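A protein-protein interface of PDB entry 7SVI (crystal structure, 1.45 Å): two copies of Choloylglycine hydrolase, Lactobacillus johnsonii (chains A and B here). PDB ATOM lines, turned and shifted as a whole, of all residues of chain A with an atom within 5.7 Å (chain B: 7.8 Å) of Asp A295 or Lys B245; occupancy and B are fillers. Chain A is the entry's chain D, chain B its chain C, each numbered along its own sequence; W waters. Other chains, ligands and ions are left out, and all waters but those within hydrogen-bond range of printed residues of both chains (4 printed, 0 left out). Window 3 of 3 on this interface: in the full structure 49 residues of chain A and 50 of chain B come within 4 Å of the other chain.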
ATOM      1  N   ASN A 291      25.651 -30.742  13.945  1.00  0.00           N
ATOM      2  CA  ASN A 291      26.026 -29.677  14.862  1.00  0.00           C
ATOM      3  C   ASN A 291      27.300 -29.027  14.347  1.00  0.00           C
ATOM      4  O   ASN A 291      27.893 -29.462  13.354  1.00  0.00           O
ATOM      5  CB  ASN A 291      26.076 -30.112  16.340  1.00  0.00           C
ATOM      6  CG  ASN A 291      27.258 -31.022  16.680  1.00  0.00           C
ATOM      7  OD1 ASN A 291      28.117 -31.325  15.849  1.00  0.00           O
ATOM      8  ND2 ASN A 291      27.293 -31.458  17.933  1.00  0.00           N
ATOM      9  N   PHE A 292      27.700 -27.951  15.003  1.00  0.00           N
ATOM     10  CA  PHE A 292      28.768 -27.112  14.498  1.00  0.00           C
ATOM     11  C   PHE A 292      29.766 -26.854  15.613  1.00  0.00           C
ATOM     12  O   PHE A 292      29.463 -27.033  16.795  1.00  0.00           O
ATOM     13  CB  PHE A 292      28.205 -25.804  13.946  1.00  0.00           C
ATOM     14  CG  PHE A 292      27.272 -26.013  12.797  1.00  0.00           C
ATOM     15  CD1 PHE A 292      25.915 -26.214  13.012  1.00  0.00           C
ATOM     16  CD2 PHE A 292      27.753 -26.058  11.504  1.00  0.00           C
ATOM     17  CE1 PHE A 292      25.048 -26.435  11.941  1.00  0.00           C
ATOM     18  CE2 PHE A 292      26.890 -26.272  10.431  1.00  0.00           C
ATOM     19  CZ  PHE A 292      25.543 -26.460  10.657  1.00  0.00           C
ATOM     20  N   GLU A 293      30.975 -26.445  15.211  1.00  0.00           N
ATOM     21  CA  GLU A 293      32.036 -26.222  16.193  1.00  0.00           C
ATOM     22  C   GLU A 293      31.615 -25.220  17.257  1.00  0.00           C
ATOM     23  O   GLU A 293      32.047 -25.326  18.411  1.00  0.00           O
ATOM     24  CB  GLU A 293      33.319 -25.750  15.506  1.00  0.00           C
ATOM     25  CG  GLU A 293      34.485 -25.482  16.470  1.00  0.00           C
ATOM     26  CD  GLU A 293      34.503 -24.064  17.020  1.00  0.00           C
ATOM     27  OE1 GLU A 293      33.913 -23.156  16.388  1.00  0.00           O
ATOM     28  OE2 GLU A 293      35.104 -23.850  18.099  1.00  0.00           O
ATOM     29  N   ASP A 294      30.782 -24.244  16.899  1.00  0.00           N
ATOM     30  CA  ASP A 294      30.388 -23.197  17.835  1.00  0.00           C
ATOM     31  C   ASP A 294      28.938 -23.318  18.294  1.00  0.00           C
ATOM     32  O   ASP A 294      28.408 -22.374  18.894  1.00  0.00           O
ATOM     33  CB  ASP A 294      30.659 -21.820  17.237  1.00  0.00           C
ATOM     34  CG  ASP A 294      29.880 -21.575  15.964  1.00  0.00           C
ATOM     35  OD1 ASP A 294      29.202 -22.508  15.477  1.00  0.00           O
ATOM     36  OD2 ASP A 294      29.950 -20.440  15.449  1.00  0.00           O
ATOM     37  N   ASP A 295      28.288 -24.453  18.034  1.00  0.00           N
ATOM     38  CA  ASP A 295      26.916 -24.680  18.488  1.00  0.00           C
ATOM     39  C   ASP A 295      26.700 -26.191  18.493  1.00  0.00           C
ATOM     40  O   ASP A 295      26.484 -26.790  17.433  1.00  0.00           O
ATOM     41  CB  ASP A 295      25.903 -23.983  17.595  1.00  0.00           C
ATOM     42  CG  ASP A 295      24.482 -24.050  18.152  1.00  0.00           C
ATOM     43  OD1 ASP A 295      24.210 -24.899  19.028  1.00  0.00           O
ATOM     44  OD2 ASP A 295      23.628 -23.257  17.695  1.00  0.00           O
ATOM     45  N   PHE A 296      26.734 -26.784  19.682  1.00  0.00           N
ATOM     46  CA  PHE A 296      26.701 -28.232  19.818  1.00  0.00           C
ATOM     47  C   PHE A 296      25.307 -28.825  19.722  1.00  0.00           C
ATOM     48  O   PHE A 296      25.184 -30.051  19.645  1.00  0.00           O
ATOM     49  CB  PHE A 296      27.346 -28.666  21.143  1.00  0.00           C
ATOM     50  CG  PHE A 296      28.059 -29.993  21.057  1.00  0.00           C
ATOM     51  CD1 PHE A 296      27.457 -31.159  21.510  1.00  0.00           C
ATOM     52  CD2 PHE A 296      29.332 -30.075  20.494  1.00  0.00           C
ATOM     53  CE1 PHE A 296      28.114 -32.384  21.417  1.00  0.00           C
ATOM     54  CE2 PHE A 296      29.988 -31.292  20.404  1.00  0.00           C
ATOM     55  CZ  PHE A 296      29.379 -32.442  20.854  1.00  0.00           C
ATOM     56  N   GLU A 297      24.262 -28.001  19.728  1.00  0.00           N
ATOM     57  CA  GLU A 297      22.908 -28.530  19.682  1.00  0.00           C
ATOM     58  C   GLU A 297      22.701 -29.314  18.394  1.00  0.00           C
ATOM     59  O   GLU A 297      23.070 -28.857  17.310  1.00  0.00           O
ATOM     60  CB  GLU A 297      21.908 -27.376  19.762  1.00  0.00           C
ATOM     61  CG  GLU A 297      20.452 -27.794  19.603  1.00  0.00           C
ATOM     62  CD  GLU A 297      19.481 -26.625  19.743  1.00  0.00           C
ATOM     63  OE1 GLU A 297      19.867 -25.588  20.322  1.00  0.00           O
ATOM     64  OE2 GLU A 297      18.328 -26.755  19.275  1.00  0.00           O
ATOM     65  N   LYS A 299      20.876 -30.293  15.390  1.00  0.00           N
ATOM     66  CA  LYS A 299      19.833 -29.731  14.540  1.00  0.00           C
ATOM     67  C   LYS A 299      19.353 -30.798  13.568  1.00  0.00           C
ATOM     68  O   LYS A 299      20.111 -31.684  13.174  1.00  0.00           O
ATOM     69  CB  LYS A 299      20.359 -28.528  13.754  1.00  0.00           C
ATOM     70  CG  LYS A 299      20.851 -27.364  14.616  1.00  0.00           C
ATOM     71  CD  LYS A 299      19.828 -26.961  15.660  1.00  0.00           C
ATOM     72  CE  LYS A 299      20.215 -25.643  16.331  1.00  0.00           C
ATOM     73  NZ  LYS A 299      21.612 -25.235  16.007  1.00  0.00           N
ATOM     74  N   TYR B  15      32.779 -22.849  32.550  1.00  0.00           N
ATOM     75  CA  TYR B  15      32.235 -24.053  31.943  1.00  0.00           C
ATOM     76  C   TYR B  15      33.028 -25.218  32.520  1.00  0.00           C
ATOM     77  O   TYR B  15      34.253 -25.263  32.377  1.00  0.00           O
ATOM     78  CB  TYR B  15      32.326 -23.955  30.412  1.00  0.00           C
ATOM     79  CG  TYR B  15      31.540 -22.750  29.939  1.00  0.00           C
ATOM     80  CD1 TYR B  15      30.206 -22.873  29.583  1.00  0.00           C
ATOM     81  CD2 TYR B  15      32.110 -21.479  29.928  1.00  0.00           C
ATOM     82  CE1 TYR B  15      29.459 -21.761  29.203  1.00  0.00           C
ATOM     83  CE2 TYR B  15      31.369 -20.357  29.558  1.00  0.00           C
ATOM     84  CZ  TYR B  15      30.047 -20.522  29.183  1.00  0.00           C
ATOM     85  OH  TYR B  15      29.282 -19.429  28.810  1.00  0.00           O
ATOM     86  N   ALA B 241      36.294 -18.678  23.398  1.00  0.00           N
ATOM     87  CA  ALA B 241      35.010 -18.649  22.719  1.00  0.00           C
ATOM     88  C   ALA B 241      34.154 -17.554  23.343  1.00  0.00           C
ATOM     89  O   ALA B 241      34.319 -17.217  24.521  1.00  0.00           O
ATOM     90  CB  ALA B 241      34.302 -19.997  22.854  1.00  0.00           C
ATOM     91  N   LYS B 242      33.248 -16.995  22.543  1.00  0.00           N
ATOM     92  CA  LYS B 242      32.370 -15.914  22.978  1.00  0.00           C
ATOM     93  C   LYS B 242      30.929 -16.405  23.029  1.00  0.00           C
ATOM     94  O   LYS B 242      30.413 -16.934  22.038  1.00  0.00           O
ATOM     95  CB  LYS B 242      32.469 -14.726  22.020  1.00  0.00           C
ATOM     96  CG  LYS B 242      33.886 -14.352  21.632  1.00  0.00           C
ATOM     97  CD  LYS B 242      33.906 -13.500  20.367  1.00  0.00           C
ATOM     98  CE  LYS B 242      35.126 -12.582  20.324  1.00  0.00           C
ATOM     99  NZ  LYS B 242      36.247 -13.075  21.181  1.00  0.00           N
ATOM    100  N   GLY B 243      30.279 -16.216  24.173  1.00  0.00           N
ATOM    101  CA  GLY B 243      28.870 -16.523  24.304  1.00  0.00           C
ATOM    102  C   GLY B 243      28.610 -17.929  24.819  1.00  0.00           C
ATOM    103  O   GLY B 243      29.465 -18.816  24.778  1.00  0.00           O
ATOM    104  N   GLU B 244      27.383 -18.126  25.304  1.00  0.00           N
ATOM    105  CA  GLU B 244      27.010 -19.394  25.925  1.00  0.00           C
ATOM    106  C   GLU B 244      27.097 -20.553  24.939  1.00  0.00           C
ATOM    107  O   GLU B 244      27.664 -21.607  25.253  1.00  0.00           O
ATOM    108  CB  GLU B 244      25.602 -19.292  26.518  1.00  0.00           C
ATOM    109  CG  GLU B 244      25.044 -20.594  27.064  1.00  0.00           C
ATOM    110  CD  GLU B 244      25.444 -20.857  28.517  1.00  0.00           C
ATOM    111  OE1 GLU B 244      26.286 -20.105  29.051  1.00  0.00           O
ATOM    112  OE2 GLU B 244      24.916 -21.815  29.113  1.00  0.00           O
ATOM    113  N   LYS B 245      26.522 -20.388  23.743  1.00  0.00           N
ATOM    114  CA  LYS B 245      26.482 -21.497  22.793  1.00  0.00           C
ATOM    115  C   LYS B 245      27.886 -21.934  22.401  1.00  0.00           C
ATOM    116  O   LYS B 245      28.193 -23.133  22.370  1.00  0.00           O
ATOM    117  CB  LYS B 245      25.694 -21.096  21.549  1.00  0.00           C
ATOM    118  CG  LYS B 245      24.190 -21.230  21.699  1.00  0.00           C
ATOM    119  CD  LYS B 245      23.486 -20.478  20.578  1.00  0.00           C
ATOM    120  CE  LYS B 245      22.059 -20.956  20.380  1.00  0.00           C
ATOM    121  NZ  LYS B 245      21.327 -21.171  21.647  1.00  0.00           N
ATOM    122  N   ALA B 246      28.750 -20.970  22.092  1.00  0.00           N
ATOM    123  CA  ALA B 246      30.090 -21.303  21.619  1.00  0.00           C
ATOM    124  C   ALA B 246      30.948 -21.905  22.724  1.00  0.00           C
ATOM    125  O   ALA B 246      31.779 -22.781  22.456  1.00  0.00           O
ATOM    126  CB  ALA B 246      30.761 -20.069  21.026  1.00  0.00           C
ATOM    127  N   ASN B 247      30.758 -21.471  23.970  1.00  0.00           N
ATOM    128  CA  ASN B 247      31.566 -22.026  25.049  1.00  0.00           C
ATOM    129  C   ASN B 247      31.106 -23.429  25.419  1.00  0.00           C
ATOM    130  O   ASN B 247      31.936 -24.311  25.673  1.00  0.00           O
ATOM    131  CB  ASN B 247      31.552 -21.092  26.259  1.00  0.00           C
ATOM    132  CG  ASN B 247      32.601 -20.008  26.160  1.00  0.00           C
ATOM    133  OD1 ASN B 247      33.784 -20.246  26.412  1.00  0.00           O
ATOM    134  ND2 ASN B 247      32.177 -18.808  25.782  1.00  0.00           N
ATOM    135  N   VAL B 248      29.791 -23.665  25.444  1.00  0.00           N
ATOM    136  CA  VAL B 248      29.287 -25.017  25.663  1.00  0.00           C
ATOM    137  C   VAL B 248      29.765 -25.941  24.547  1.00  0.00           C
ATOM    138  O   VAL B 248      30.159 -27.091  24.789  1.00  0.00           O
ATOM    139  CB  VAL B 248      27.750 -24.999  25.778  1.00  0.00           C
ATOM    140  CG1 VAL B 248      27.180 -26.409  25.791  1.00  0.00           C
ATOM    141  CG2 VAL B 248      27.326 -24.242  27.035  1.00  0.00           C
ATOM    142  N   ALA B 249      29.747 -25.442  23.308  1.00  0.00           N
ATOM    143  CA  ALA B 249      30.193 -26.249  22.173  1.00  0.00           C
ATOM    144  C   ALA B 249      31.670 -26.587  22.297  1.00  0.00           C
ATOM    145  O   ALA B 249      32.059 -27.754  22.167  1.00  0.00           O
ATOM    146  CB  ALA B 249      29.907 -25.507  20.869  1.00  0.00           C
ATOM    147  N   LYS B 250      32.502 -25.575  22.565  1.00  0.00           N
ATOM    148  CA  LYS B 250      33.924 -25.796  22.827  1.00  0.00           C
ATOM    149  C   LYS B 250      34.129 -26.876  23.882  1.00  0.00           C
ATOM    150  O   LYS B 250      34.960 -27.781  23.722  1.00  0.00           O
ATOM    151  CB  LYS B 250      34.559 -24.475  23.277  1.00  0.00           C
ATOM    152  CG  LYS B 250      35.926 -24.610  23.949  1.00  0.00           C
ATOM    153  CD  LYS B 250      36.484 -23.237  24.341  1.00  0.00           C
ATOM    154  CE  LYS B 250      37.744 -23.362  25.211  1.00  0.00           C
ATOM    155  NZ  LYS B 250      38.427 -22.037  25.351  1.00  0.00           N
ATOM    156  N   PHE B 251      33.365 -26.794  24.972  1.00  0.00           N
ATOM    157  CA  PHE B 251      33.489 -27.756  26.061  1.00  0.00           C
ATOM    158  C   PHE B 251      33.188 -29.174  25.584  1.00  0.00           C
ATOM    159  O   PHE B 251      33.968 -30.106  25.821  1.00  0.00           O
ATOM    160  CB  PHE B 251      32.542 -27.340  27.195  1.00  0.00           C
ATOM    161  CG  PHE B 251      32.621 -28.222  28.403  1.00  0.00           C
ATOM    162  CD1 PHE B 251      31.918 -29.416  28.458  1.00  0.00           C
ATOM    163  CD2 PHE B 251      33.429 -27.867  29.477  1.00  0.00           C
ATOM    164  CE1 PHE B 251      32.005 -30.241  29.569  1.00  0.00           C
ATOM    165  CE2 PHE B 251      33.525 -28.681  30.591  1.00  0.00           C
ATOM    166  CZ  PHE B 251      32.815 -29.869  30.642  1.00  0.00           C
ATOM    167  N   PHE B 252      32.041 -29.363  24.920  1.00  0.00           N
ATOM    168  CA  PHE B 252      31.698 -30.692  24.426  1.00  0.00           C
ATOM    169  C   PHE B 252      32.643 -31.148  23.320  1.00  0.00           C
ATOM    170  O   PHE B 252      32.893 -32.349  23.190  1.00  0.00           O
ATOM    171  CB  PHE B 252      30.240 -30.743  23.952  1.00  0.00           C
ATOM    172  CG  PHE B 252      29.259 -31.003  25.062  1.00  0.00           C
ATOM    173  CD1 PHE B 252      28.862 -29.976  25.906  1.00  0.00           C
ATOM    174  CD2 PHE B 252      28.756 -32.269  25.280  1.00  0.00           C
ATOM    175  CE1 PHE B 252      27.967 -30.216  26.934  1.00  0.00           C
ATOM    176  CE2 PHE B 252      27.864 -32.516  26.299  1.00  0.00           C
ATOM    177  CZ  PHE B 252      27.476 -31.485  27.143  1.00  0.00           C
ATOM    178  N   ASN B 253      33.183 -30.215  22.531  1.00  0.00           N
ATOM    179  CA  ASN B 253      34.155 -30.605  21.508  1.00  0.00           C
ATOM    180  C   ASN B 253      35.361 -31.282  22.148  1.00  0.00           C
ATOM    181  O   ASN B 253      35.817 -32.338  21.687  1.00  0.00           O
ATOM    182  CB  ASN B 253      34.615 -29.382  20.716  1.00  0.00           C
ATOM    183  CG  ASN B 253      33.523 -28.805  19.826  1.00  0.00           C
ATOM    184  OD1 ASN B 253      32.598 -29.518  19.408  1.00  0.00           O
ATOM    185  ND2 ASN B 253      33.634 -27.518  19.518  1.00  0.00           N
ATOM    186  N   SER B 282      27.310 -24.501  33.191  1.00  0.00           N
ATOM    187  CA  SER B 282      27.610 -23.107  32.889  1.00  0.00           C
ATOM    188  C   SER B 282      27.200 -22.257  34.089  1.00  0.00           C
ATOM    189  O   SER B 282      26.006 -22.121  34.376  1.00  0.00           O
ATOM    190  CB  SER B 282      26.834 -22.643  31.660  1.00  0.00           C
ATOM    191  OG  SER B 282      27.002 -21.250  31.455  1.00  0.00           O
ATOM    192  N   TYR B 289      24.152 -28.985  31.286  1.00  0.00           N
ATOM    193  CA  TYR B 289      23.938 -29.607  29.984  1.00  0.00           C
ATOM    194  C   TYR B 289      24.454 -31.034  30.026  1.00  0.00           C
ATOM    195  O   TYR B 289      25.506 -31.300  30.614  1.00  0.00           O
ATOM    196  CB  TYR B 289      24.763 -28.885  28.921  1.00  0.00           C
ATOM    197  CG  TYR B 289      24.387 -27.464  28.642  1.00  0.00           C
ATOM    198  CD1 TYR B 289      24.856 -26.432  29.442  1.00  0.00           C
ATOM    199  CD2 TYR B 289      23.605 -27.140  27.541  1.00  0.00           C
ATOM    200  CE1 TYR B 289      24.527 -25.123  29.185  1.00  0.00           C
ATOM    201  CE2 TYR B 289      23.268 -25.830  27.268  1.00  0.00           C
ATOM    202  CZ  TYR B 289      23.731 -24.823  28.091  1.00  0.00           C
ATOM    203  OH  TYR B 289      23.413 -23.517  27.820  1.00  0.00           O
ATOM    204  N   LEU B 298      21.403 -32.728  23.386  1.00  0.00           N
ATOM    205  CA  LEU B 298      21.853 -31.934  24.528  1.00  0.00           C
ATOM    206  C   LEU B 298      20.643 -31.563  25.381  1.00  0.00           C
ATOM    207  O   LEU B 298      19.825 -30.726  24.979  1.00  0.00           O
ATOM    208  CB  LEU B 298      22.538 -30.672  24.017  1.00  0.00           C
ATOM    209  CG  LEU B 298      23.713 -30.104  24.803  1.00  0.00           C
ATOM    210  CD1 LEU B 298      24.741 -31.184  25.048  1.00  0.00           C
ATOM    211  CD2 LEU B 298      24.319 -28.935  24.041  1.00  0.00           C
HETATM  212  O   HOH W   1      26.485 -25.345  22.167  1.00  0.00           O
HETATM  213  O   HOH W   2      33.152 -22.727  20.038  1.00  0.00           O
HETATM  214  O   HOH W   3      30.825 -29.408  17.313  1.00  0.00           O
HETATM  215  O   HOH W   4      22.329 -24.092  20.854  1.00  0.00           O
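The side-chain amide nitrogen of Asn B253 lies within hydrogen-bond range of the backbone carbonyl oxygen of Glu A293 (2.9 Å).
N of Glu A297 sits at hydrogen-bond distance from OD1 of Asp A295 (3.2 Å). The side-chain carboxylate of Asp A295 is in salt-bridge range of the side-chain amino group of Lys A299. The backbone carbonyl oxygen (O) of Ala B249 lies close to the side-chain amide nitrogen (ND2) of Asn B253 (3.1 Å). ND2 of Asn A291 lies within hydrogen-bond range of O of Phe A296.
Among the printed residues, merely in contact across the chains: Glu A293 with Ala B249 (3.3 Å), Phe A296 with Asn B253 (3.3 Å), Asp A294 with Ala B246 (3.4 Å), Asp A295 with Ala B249 (3.4 Å), Asp A294 with Ala B249 (3.5 Å), Asp A294 with Lys B245 (3.6 Å), Phe A296 with Phe B252 (3.6 Å), Phe A296 with Ala B249 (3.6 Å) and Asp A295 with Lys B245 (3.9 Å).
Of chain B, only Lys B245 and Ala B249 come within 4 Å of Asp A295. Of chain A, only Asp A294 (3.6 Å) and Asp A295 (3.9 Å) come within 4 Å of Lys B245. Of the printed residues of chain B, Asp A294 touches Lys B245, Ala B246 and Ala B249. Of the printed residues of chain B, Glu A293 touches Ala B249 (3.3 Å) and Asn B253 (2.9 Å). Of the printed residues of chain A, Ala B249 touches Glu A293 (3.3 Å), Asp A294 (3.5 Å), Asp A295 (3.4 Å) and Phe A296 (3.6 Å). Of the printed residues of chain A, Ala B246 touches Asp A294 (3.4 Å). The nearest residue of chain A that does not touch Lys B245 is Phe A296 (4.8 Å). The nearest printed residue of chain B that does not touch Glu A293 is Lys B250 (4.2 Å).
Of the 17 printed residues of chain B, 5 touch a printed residue of chain A. Hydrophobic or aromatic side chains of chain B that line the printed part of chain A: Ala B246, Ala B249 and Phe B252. Among the printed residues, 10 pairs touch across the chains.
No position is printed for both chains. Of the 10 pairs that touch across the chains among the printed residues, none has its exchanged pair printed and touching as well.
Water W4 lies within hydrogen-bond range of OD1 of Asp A295, OE1 of Glu A297 and NZ of Lys B245. Water W3 bridges OD1 of Asn B253 (2.7 Å) and O of Phe A292 (2.8 Å). Water W2 bridges O of Ala B246 (2.8 Å) and OE2 of Glu A293 (3.0 Å). Water W1 lies within hydrogen-bond range of the backbone carbonyl oxygen of Lys B245 (2.8 Å), the backbone NH of Phe A296 (2.9 Å) and the backbone NH of Ala B249 (3.5 Å).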
